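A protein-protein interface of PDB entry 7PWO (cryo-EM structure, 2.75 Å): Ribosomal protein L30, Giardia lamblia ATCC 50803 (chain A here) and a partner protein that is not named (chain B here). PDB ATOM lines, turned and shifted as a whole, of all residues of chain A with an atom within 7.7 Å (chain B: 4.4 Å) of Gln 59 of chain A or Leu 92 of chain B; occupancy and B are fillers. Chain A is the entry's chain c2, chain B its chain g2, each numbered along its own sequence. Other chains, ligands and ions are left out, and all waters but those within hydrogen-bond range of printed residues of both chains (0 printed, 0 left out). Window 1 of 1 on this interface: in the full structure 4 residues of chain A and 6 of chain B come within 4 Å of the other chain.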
ATOM      1  N   THR A  31     -19.814 -10.095  21.268  1.00  0.00           N
ATOM      2  CA  THR A  31     -19.799  -9.132  20.175  1.00  0.00           C
ATOM      3  C   THR A  31     -21.162  -9.023  19.499  1.00  0.00           C
ATOM      4  O   THR A  31     -21.585  -7.926  19.122  1.00  0.00           O
ATOM      5  CB  THR A  31     -18.717  -9.532  19.171  1.00  0.00           C
ATOM      6  OG1 THR A  31     -17.429  -9.223  19.706  1.00  0.00           O
ATOM      7  CG2 THR A  31     -18.874  -8.797  17.857  1.00  0.00           C
ATOM      8  N   ASP A  32     -21.860 -10.149  19.327  1.00  0.00           N
ATOM      9  CA  ASP A  32     -23.136 -10.133  18.613  1.00  0.00           C
ATOM     10  C   ASP A  32     -24.184  -9.325  19.376  1.00  0.00           C
ATOM     11  O   ASP A  32     -24.843  -8.438  18.808  1.00  0.00           O
ATOM     12  CB  ASP A  32     -23.615 -11.564  18.369  1.00  0.00           C
ATOM     13  CG  ASP A  32     -22.924 -12.222  17.178  1.00  0.00           C
ATOM     14  OD1 ASP A  32     -22.540 -11.511  16.230  1.00  0.00           O
ATOM     15  OD2 ASP A  32     -22.767 -13.459  17.182  1.00  0.00           O
ATOM     16  N   ILE A  35     -23.336  -5.594  19.167  1.00  0.00           N
ATOM     17  CA  ILE A  35     -23.812  -4.946  17.945  1.00  0.00           C
ATOM     18  C   ILE A  35     -25.309  -4.675  18.012  1.00  0.00           C
ATOM     19  O   ILE A  35     -25.768  -3.577  17.672  1.00  0.00           O
ATOM     20  CB  ILE A  35     -23.466  -5.782  16.702  1.00  0.00           C
ATOM     21  CG1 ILE A  35     -21.953  -5.892  16.526  1.00  0.00           C
ATOM     22  CG2 ILE A  35     -24.157  -5.222  15.475  1.00  0.00           C
ATOM     23  CD1 ILE A  35     -21.553  -6.885  15.502  1.00  0.00           C
ATOM     24  N   ILE A  38     -25.961  -1.772  20.404  1.00  0.00           N
ATOM     25  CA  ILE A  38     -25.514  -0.479  19.888  1.00  0.00           C
ATOM     26  C   ILE A  38     -26.436   0.008  18.777  1.00  0.00           C
ATOM     27  O   ILE A  38     -26.703   1.211  18.670  1.00  0.00           O
ATOM     28  CB  ILE A  38     -24.048  -0.530  19.421  1.00  0.00           C
ATOM     29  CG1 ILE A  38     -23.112  -0.761  20.601  1.00  0.00           C
ATOM     30  CG2 ILE A  38     -23.647   0.775  18.752  1.00  0.00           C
ATOM     31  CD1 ILE A  38     -21.803  -1.392  20.222  1.00  0.00           C
ATOM     32  N   PRO A  53     -10.106  -8.572  17.800  1.00  0.00           N
ATOM     33  CA  PRO A  53      -9.688  -8.655  16.392  1.00  0.00           C
ATOM     34  C   PRO A  53      -9.878  -7.322  15.692  1.00  0.00           C
ATOM     35  O   PRO A  53     -10.908  -6.656  15.880  1.00  0.00           O
ATOM     36  CB  PRO A  53     -10.612  -9.733  15.815  1.00  0.00           C
ATOM     37  CG  PRO A  53     -10.978 -10.559  16.976  1.00  0.00           C
ATOM     38  CD  PRO A  53     -11.071  -9.625  18.148  1.00  0.00           C
ATOM     39  N   PRO A  54      -8.900  -6.896  14.885  1.00  0.00           N
ATOM     40  CA  PRO A  54      -8.886  -5.495  14.424  1.00  0.00           C
ATOM     41  C   PRO A  54     -10.040  -5.111  13.504  1.00  0.00           C
ATOM     42  O   PRO A  54     -10.515  -3.973  13.595  1.00  0.00           O
ATOM     43  CB  PRO A  54      -7.525  -5.369  13.725  1.00  0.00           C
ATOM     44  CG  PRO A  54      -7.052  -6.780  13.494  1.00  0.00           C
ATOM     45  CD  PRO A  54      -7.651  -7.608  14.568  1.00  0.00           C
ATOM     46  N   LEU A  55     -10.525  -6.007  12.642  1.00  0.00           N
ATOM     47  CA  LEU A  55     -11.706  -5.688  11.838  1.00  0.00           C
ATOM     48  C   LEU A  55     -12.942  -5.519  12.715  1.00  0.00           C
ATOM     49  O   LEU A  55     -13.762  -4.611  12.497  1.00  0.00           O
ATOM     50  CB  LEU A  55     -11.945  -6.778  10.795  1.00  0.00           C
ATOM     51  CG  LEU A  55     -12.856  -6.457   9.606  1.00  0.00           C
ATOM     52  CD1 LEU A  55     -12.546  -5.078   9.027  1.00  0.00           C
ATOM     53  CD2 LEU A  55     -12.750  -7.538   8.540  1.00  0.00           C
ATOM     54  N   VAL A  56     -13.089  -6.385  13.715  1.00  0.00           N
ATOM     55  CA  VAL A  56     -14.219  -6.284  14.627  1.00  0.00           C
ATOM     56  C   VAL A  56     -14.152  -4.972  15.391  1.00  0.00           C
ATOM     57  O   VAL A  56     -15.158  -4.272  15.539  1.00  0.00           O
ATOM     58  CB  VAL A  56     -14.230  -7.497  15.572  1.00  0.00           C
ATOM     59  CG1 VAL A  56     -15.332  -7.375  16.596  1.00  0.00           C
ATOM     60  CG2 VAL A  56     -14.308  -8.798  14.777  1.00  0.00           C
ATOM     61  N   LYS A  57     -12.953  -4.616  15.862  1.00  0.00           N
ATOM     62  CA  LYS A  57     -12.730  -3.340  16.534  1.00  0.00           C
ATOM     63  C   LYS A  57     -13.092  -2.161  15.644  1.00  0.00           C
ATOM     64  O   LYS A  57     -13.716  -1.196  16.101  1.00  0.00           O
ATOM     65  CB  LYS A  57     -11.267  -3.234  16.962  1.00  0.00           C
ATOM     66  CG  LYS A  57     -10.953  -1.989  17.757  1.00  0.00           C
ATOM     67  CD  LYS A  57      -9.523  -1.971  18.221  1.00  0.00           C
ATOM     68  CE  LYS A  57      -9.223  -0.707  19.013  1.00  0.00           C
ATOM     69  NZ  LYS A  57      -7.828  -0.654  19.485  1.00  0.00           N
ATOM     70  N   SER A  58     -12.680  -2.205  14.376  1.00  0.00           N
ATOM     71  CA  SER A  58     -12.991  -1.117  13.459  1.00  0.00           C
ATOM     72  C   SER A  58     -14.490  -0.927  13.324  1.00  0.00           C
ATOM     73  O   SER A  58     -14.995   0.199  13.448  1.00  0.00           O
ATOM     74  CB  SER A  58     -12.356  -1.375  12.096  1.00  0.00           C
ATOM     75  OG  SER A  58     -10.947  -1.381  12.190  1.00  0.00           O
ATOM     76  N   GLN A  59     -15.233  -2.016  13.086  1.00  0.00           N
ATOM     77  CA  GLN A  59     -16.670  -1.820  12.922  1.00  0.00           C
ATOM     78  C   GLN A  59     -17.350  -1.420  14.223  1.00  0.00           C
ATOM     79  O   GLN A  59     -18.332  -0.669  14.188  1.00  0.00           O
ATOM     80  CB  GLN A  59     -17.378  -3.039  12.349  1.00  0.00           C
ATOM     81  CG  GLN A  59     -17.459  -4.231  13.229  1.00  0.00           C
ATOM     82  CD  GLN A  59     -18.138  -5.364  12.529  1.00  0.00           C
ATOM     83  OE1 GLN A  59     -18.835  -5.150  11.539  1.00  0.00           O
ATOM     84  NE2 GLN A  59     -17.930  -6.579  13.013  1.00  0.00           N
ATOM     85  N   VAL A  60     -16.864  -1.893  15.375  1.00  0.00           N
ATOM     86  CA  VAL A  60     -17.469  -1.470  16.637  1.00  0.00           C
ATOM     87  C   VAL A  60     -17.278   0.025  16.833  1.00  0.00           C
ATOM     88  O   VAL A  60     -18.221   0.747  17.173  1.00  0.00           O
ATOM     89  CB  VAL A  60     -16.904  -2.270  17.826  1.00  0.00           C
ATOM     90  CG1 VAL A  60     -17.453  -1.720  19.121  1.00  0.00           C
ATOM     91  CG2 VAL A  60     -17.276  -3.732  17.718  1.00  0.00           C
ATOM     92  N   ASP A  61     -16.056   0.513  16.610  1.00  0.00           N
ATOM     93  CA  ASP A  61     -15.777   1.935  16.783  1.00  0.00           C
ATOM     94  C   ASP A  61     -16.590   2.786  15.815  1.00  0.00           C
ATOM     95  O   ASP A  61     -17.056   3.871  16.175  1.00  0.00           O
ATOM     96  CB  ASP A  61     -14.288   2.206  16.587  1.00  0.00           C
ATOM     97  CG  ASP A  61     -13.492   2.053  17.866  1.00  0.00           C
ATOM     98  OD1 ASP A  61     -14.020   2.390  18.943  1.00  0.00           O
ATOM     99  OD2 ASP A  61     -12.333   1.593  17.789  1.00  0.00           O
ATOM    100  N   TYR A  62     -16.758   2.315  14.576  1.00  0.00           N
ATOM    101  CA  TYR A  62     -17.553   3.063  13.604  1.00  0.00           C
ATOM    102  C   TYR A  62     -19.022   3.120  14.013  1.00  0.00           C
ATOM    103  O   TYR A  62     -19.643   4.199  14.024  1.00  0.00           O
ATOM    104  CB  TYR A  62     -17.396   2.436  12.218  1.00  0.00           C
ATOM    105  CG  TYR A  62     -17.881   3.319  11.096  1.00  0.00           C
ATOM    106  CD1 TYR A  62     -17.045   4.271  10.521  1.00  0.00           C
ATOM    107  CD2 TYR A  62     -19.180   3.220  10.626  1.00  0.00           C
ATOM    108  CE1 TYR A  62     -17.492   5.090   9.506  1.00  0.00           C
ATOM    109  CE2 TYR A  62     -19.629   4.028   9.611  1.00  0.00           C
ATOM    110  CZ  TYR A  62     -18.786   4.961   9.054  1.00  0.00           C
ATOM    111  OH  TYR A  62     -19.253   5.757   8.037  1.00  0.00           O
ATOM    112  N   LEU A  63     -19.594   1.962  14.350  1.00  0.00           N
ATOM    113  CA  LEU A  63     -20.971   1.919  14.819  1.00  0.00           C
ATOM    114  C   LEU A  63     -21.164   2.812  16.040  1.00  0.00           C
ATOM    115  O   LEU A  63     -22.197   3.473  16.176  1.00  0.00           O
ATOM    116  CB  LEU A  63     -21.355   0.477  15.139  1.00  0.00           C
ATOM    117  CG  LEU A  63     -21.891  -0.424  14.025  1.00  0.00           C
ATOM    118  CD1 LEU A  63     -22.247  -1.777  14.589  1.00  0.00           C
ATOM    119  CD2 LEU A  63     -23.094   0.198  13.347  1.00  0.00           C
ATOM    120  N   CYS A  64     -20.169   2.864  16.927  1.00  0.00           N
ATOM    121  CA  CYS A  64     -20.280   3.696  18.121  1.00  0.00           C
ATOM    122  C   CYS A  64     -20.164   5.177  17.792  1.00  0.00           C
ATOM    123  O   CYS A  64     -20.820   6.004  18.429  1.00  0.00           O
ATOM    124  CB  CYS A  64     -19.238   3.289  19.163  1.00  0.00           C
ATOM    125  SG  CYS A  64     -19.467   1.636  19.854  1.00  0.00           S
ATOM    126  N   HIS A  65     -19.325   5.540  16.821  1.00  0.00           N
ATOM    127  CA  HIS A  65     -19.265   6.936  16.394  1.00  0.00           C
ATOM    128  C   HIS A  65     -20.600   7.404  15.833  1.00  0.00           C
ATOM    129  O   HIS A  65     -20.977   8.566  16.015  1.00  0.00           O
ATOM    130  CB  HIS A  65     -18.154   7.128  15.361  1.00  0.00           C
ATOM    131  CG  HIS A  65     -18.144   8.487  14.735  1.00  0.00           C
ATOM    132  ND1 HIS A  65     -18.994   8.835  13.709  1.00  0.00           N
ATOM    133  CD2 HIS A  65     -17.393   9.583  14.993  1.00  0.00           C
ATOM    134  CE1 HIS A  65     -18.770  10.090  13.363  1.00  0.00           C
ATOM    135  NE2 HIS A  65     -17.806  10.568  14.130  1.00  0.00           N
ATOM    136  N   LEU A  66     -21.318   6.527  15.134  1.00  0.00           N
ATOM    137  CA  LEU A  66     -22.661   6.896  14.686  1.00  0.00           C
ATOM    138  C   LEU A  66     -23.690   6.867  15.806  1.00  0.00           C
ATOM    139  O   LEU A  66     -24.686   7.593  15.742  1.00  0.00           O
ATOM    140  CB  LEU A  66     -23.119   6.002  13.542  1.00  0.00           C
ATOM    141  CG  LEU A  66     -22.578   6.305  12.154  1.00  0.00           C
ATOM    142  CD1 LEU A  66     -21.131   5.966  12.018  1.00  0.00           C
ATOM    143  CD2 LEU A  66     -23.397   5.492  11.182  1.00  0.00           C
ATOM    144  N   LEU B  88     -16.330  -5.611   4.523  1.00  0.00           N
ATOM    145  CA  LEU B  88     -16.106  -4.773   5.697  1.00  0.00           C
ATOM    146  C   LEU B  88     -14.751  -4.084   5.630  1.00  0.00           C
ATOM    147  O   LEU B  88     -14.646  -2.887   5.916  1.00  0.00           O
ATOM    148  CB  LEU B  88     -16.216  -5.600   6.977  1.00  0.00           C
ATOM    149  CG  LEU B  88     -17.550  -5.590   7.719  1.00  0.00           C
ATOM    150  CD1 LEU B  88     -18.657  -6.000   6.794  1.00  0.00           C
ATOM    151  CD2 LEU B  88     -17.520  -6.508   8.926  1.00  0.00           C
ATOM    152  N   GLU B  89     -13.699  -4.823   5.263  1.00  0.00           N
ATOM    153  CA  GLU B  89     -12.379  -4.218   5.133  1.00  0.00           C
ATOM    154  C   GLU B  89     -12.408  -3.036   4.181  1.00  0.00           C
ATOM    155  O   GLU B  89     -11.965  -1.935   4.525  1.00  0.00           O
ATOM    156  CB  GLU B  89     -11.362  -5.243   4.645  1.00  0.00           C
ATOM    157  CG  GLU B  89     -10.883  -6.210   5.676  1.00  0.00           C
ATOM    158  CD  GLU B  89      -9.606  -5.755   6.327  1.00  0.00           C
ATOM    159  OE1 GLU B  89      -9.345  -6.164   7.473  1.00  0.00           O
ATOM    160  OE2 GLU B  89      -8.873  -4.970   5.693  1.00  0.00           O
ATOM    161  N   SER B  90     -12.943  -3.246   2.975  1.00  0.00           N
ATOM    162  CA  SER B  90     -12.954  -2.183   1.976  1.00  0.00           C
ATOM    163  C   SER B  90     -13.702  -0.952   2.482  1.00  0.00           C
ATOM    164  O   SER B  90     -13.175   0.169   2.448  1.00  0.00           O
ATOM    165  CB  SER B  90     -13.564  -2.702   0.674  1.00  0.00           C
ATOM    166  OG  SER B  90     -13.973  -1.644  -0.172  1.00  0.00           O
ATOM    167  N   PHE B  91     -14.925  -1.142   2.988  1.00  0.00           N
ATOM    168  CA  PHE B  91     -15.729   0.009   3.392  1.00  0.00           C
ATOM    169  C   PHE B  91     -15.110   0.751   4.573  1.00  0.00           C
ATOM    170  O   PHE B  91     -14.986   1.984   4.551  1.00  0.00           O
ATOM    171  CB  PHE B  91     -17.147  -0.424   3.744  1.00  0.00           C
ATOM    172  CG  PHE B  91     -17.928   0.640   4.441  1.00  0.00           C
ATOM    173  CD1 PHE B  91     -18.219   1.832   3.798  1.00  0.00           C
ATOM    174  CD2 PHE B  91     -18.345   0.472   5.750  1.00  0.00           C
ATOM    175  CE1 PHE B  91     -18.925   2.823   4.443  1.00  0.00           C
ATOM    176  CE2 PHE B  91     -19.058   1.456   6.393  1.00  0.00           C
ATOM    177  CZ  PHE B  91     -19.345   2.635   5.742  1.00  0.00           C
ATOM    178  N   LEU B  92     -14.732   0.026   5.627  1.00  0.00           N
ATOM    179  CA  LEU B  92     -14.217   0.704   6.810  1.00  0.00           C
ATOM    180  C   LEU B  92     -12.874   1.358   6.537  1.00  0.00           C
ATOM    181  O   LEU B  92     -12.572   2.410   7.114  1.00  0.00           O
ATOM    182  CB  LEU B  92     -14.096  -0.273   7.974  1.00  0.00           C
ATOM    183  CG  LEU B  92     -15.379  -0.740   8.645  1.00  0.00           C
ATOM    184  CD1 LEU B  92     -15.099  -2.011   9.424  1.00  0.00           C
ATOM    185  CD2 LEU B  92     -15.944   0.340   9.551  1.00  0.00           C
ATOM    186  N   ASN B  93     -12.053   0.769   5.668  1.00  0.00           N
ATOM    187  CA  ASN B  93     -10.787   1.411   5.346  1.00  0.00           C
ATOM    188  C   ASN B  93     -11.007   2.675   4.530  1.00  0.00           C
ATOM    189  O   ASN B  93     -10.298   3.665   4.723  1.00  0.00           O
ATOM    190  CB  ASN B  93      -9.872   0.429   4.618  1.00  0.00           C
ATOM    191  CG  ASN B  93      -9.287  -0.614   5.549  1.00  0.00           C
ATOM    192  OD1 ASN B  93      -9.470  -0.545   6.767  1.00  0.00           O
ATOM    193  ND2 ASN B  93      -8.576  -1.590   4.981  1.00  0.00           N
ATOM    194  N   GLU B  94     -11.982   2.666   3.614  1.00  0.00           N
ATOM    195  CA  GLU B  94     -12.376   3.910   2.958  1.00  0.00           C
ATOM    196  C   GLU B  94     -12.756   4.975   3.985  1.00  0.00           C
ATOM    197  O   GLU B  94     -12.338   6.138   3.887  1.00  0.00           O
ATOM    198  CB  GLU B  94     -13.542   3.650   2.016  1.00  0.00           C
ATOM    199  CG  GLU B  94     -14.047   4.885   1.324  1.00  0.00           C
ATOM    200  CD  GLU B  94     -15.270   4.612   0.484  1.00  0.00           C
ATOM    201  OE1 GLU B  94     -15.104   4.254  -0.699  1.00  0.00           O
ATOM    202  OE2 GLU B  94     -16.395   4.765   1.004  1.00  0.00           O
ATOM    203  N   GLU B  95     -13.557   4.579   4.978  1.00  0.00           N
ATOM    204  CA  GLU B  95     -14.007   5.508   6.012  1.00  0.00           C
ATOM    205  C   GLU B  95     -12.847   6.069   6.830  1.00  0.00           C
ATOM    206  O   GLU B  95     -12.887   7.228   7.256  1.00  0.00           O
ATOM    207  CB  GLU B  95     -15.011   4.820   6.930  1.00  0.00           C
ATOM    208  CG  GLU B  95     -16.296   4.461   6.258  1.00  0.00           C
ATOM    209  CD  GLU B  95     -17.077   5.690   5.849  1.00  0.00           C
ATOM    210  OE1 GLU B  95     -16.979   6.722   6.554  1.00  0.00           O
ATOM    211  OE2 GLU B  95     -17.786   5.631   4.823  1.00  0.00           O
ATOM    212  N   ASN B  96     -11.841   5.255   7.120  1.00  0.00           N
ATOM    213  CA  ASN B  96     -10.715   5.749   7.904  1.00  0.00           C
ATOM    214  C   ASN B  96      -9.602   6.363   7.062  1.00  0.00           C
ATOM    215  O   ASN B  96      -8.670   6.943   7.628  1.00  0.00           O
ATOM    216  CB  ASN B  96     -10.139   4.635   8.782  1.00  0.00           C
ATOM    217  CG  ASN B  96     -11.126   4.151   9.811  1.00  0.00           C
ATOM    218  OD1 ASN B  96     -11.571   3.009   9.780  1.00  0.00           O
ATOM    219  ND2 ASN B  96     -11.482   5.030  10.735  1.00  0.00           N
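The side-chain carboxylate (OE1) of Glu 95 of chain B sits at hydrogen-bond distance from the side-chain hydroxyl (OH) of Tyr 62 of chain A, at 2.9 Å.
O of Pro 54 of chain A sits at hydrogen-bond distance from OG of Ser 58 of chain A (3.0 Å). ND2 of Asn 93 of chain B lies close to O of Glu 89 of chain B, at 3.4 Å. O of Leu 92 of chain B lies close to OD1 of Asn 96 of chain B (2.9 Å).
CG of Glu 89 of chain B touches CD2 of Leu 55 of chain A (3.7 Å). Ser 58 of chain A touches Leu 92 of chain B (CB to CD1, 3.9 Å). Gln 59 of chain A touches Leu 88 of chain B (OE1 to CD2, 3.2 Å). Leu 92 of chain B touches Gln 59 of chain A. Phe 91 of chain B touches Tyr 62 of chain A. Tyr 62 of chain A touches Leu 92 of chain B (CB to CD2, 3.7 Å).
Pro 53 of chain A touches none of the printed residues of chain B. Printed residues of chain B within 4 Å of Leu 55 of chain A: Glu 89. Printed residues of chain B within 4 Å of Gln 59 of chain A: Leu 88 (3.2 Å) and Leu 92 (3.7 Å). Leu 66 of chain A touches none of the printed residues of chain B. Of the printed residues of chain A, Leu 88 of chain B touches Gln 59 (3.2 Å). Printed residues of chain A within 4 Å of Glu 89 of chain B: Leu 55. Printed residues of chain A within 4 Å of Leu 92 of chain B: Ser 58 (3.9 Å), Gln 59 (3.7 Å) and Tyr 62 (3.7 Å). Of the printed residues of chain A, Glu 95 of chain B touches Tyr 62 (2.9 Å). The nearest printed residue of chain A that does not touch Leu 92 of chain B is Leu 55 of chain A (4.01 Å).
Of the 9 printed residues of chain B, 5 touch a printed residue of chain A. Hydrophobic or aromatic side chains of chain B within 4 Å of the printed part of chain A: Leu 88, Phe 91 and Leu 92. Among the printed residues, no Asp or Glu carboxylate lies within 4 Å of a Lys or Arg side-chain nitrogen of the other chain.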
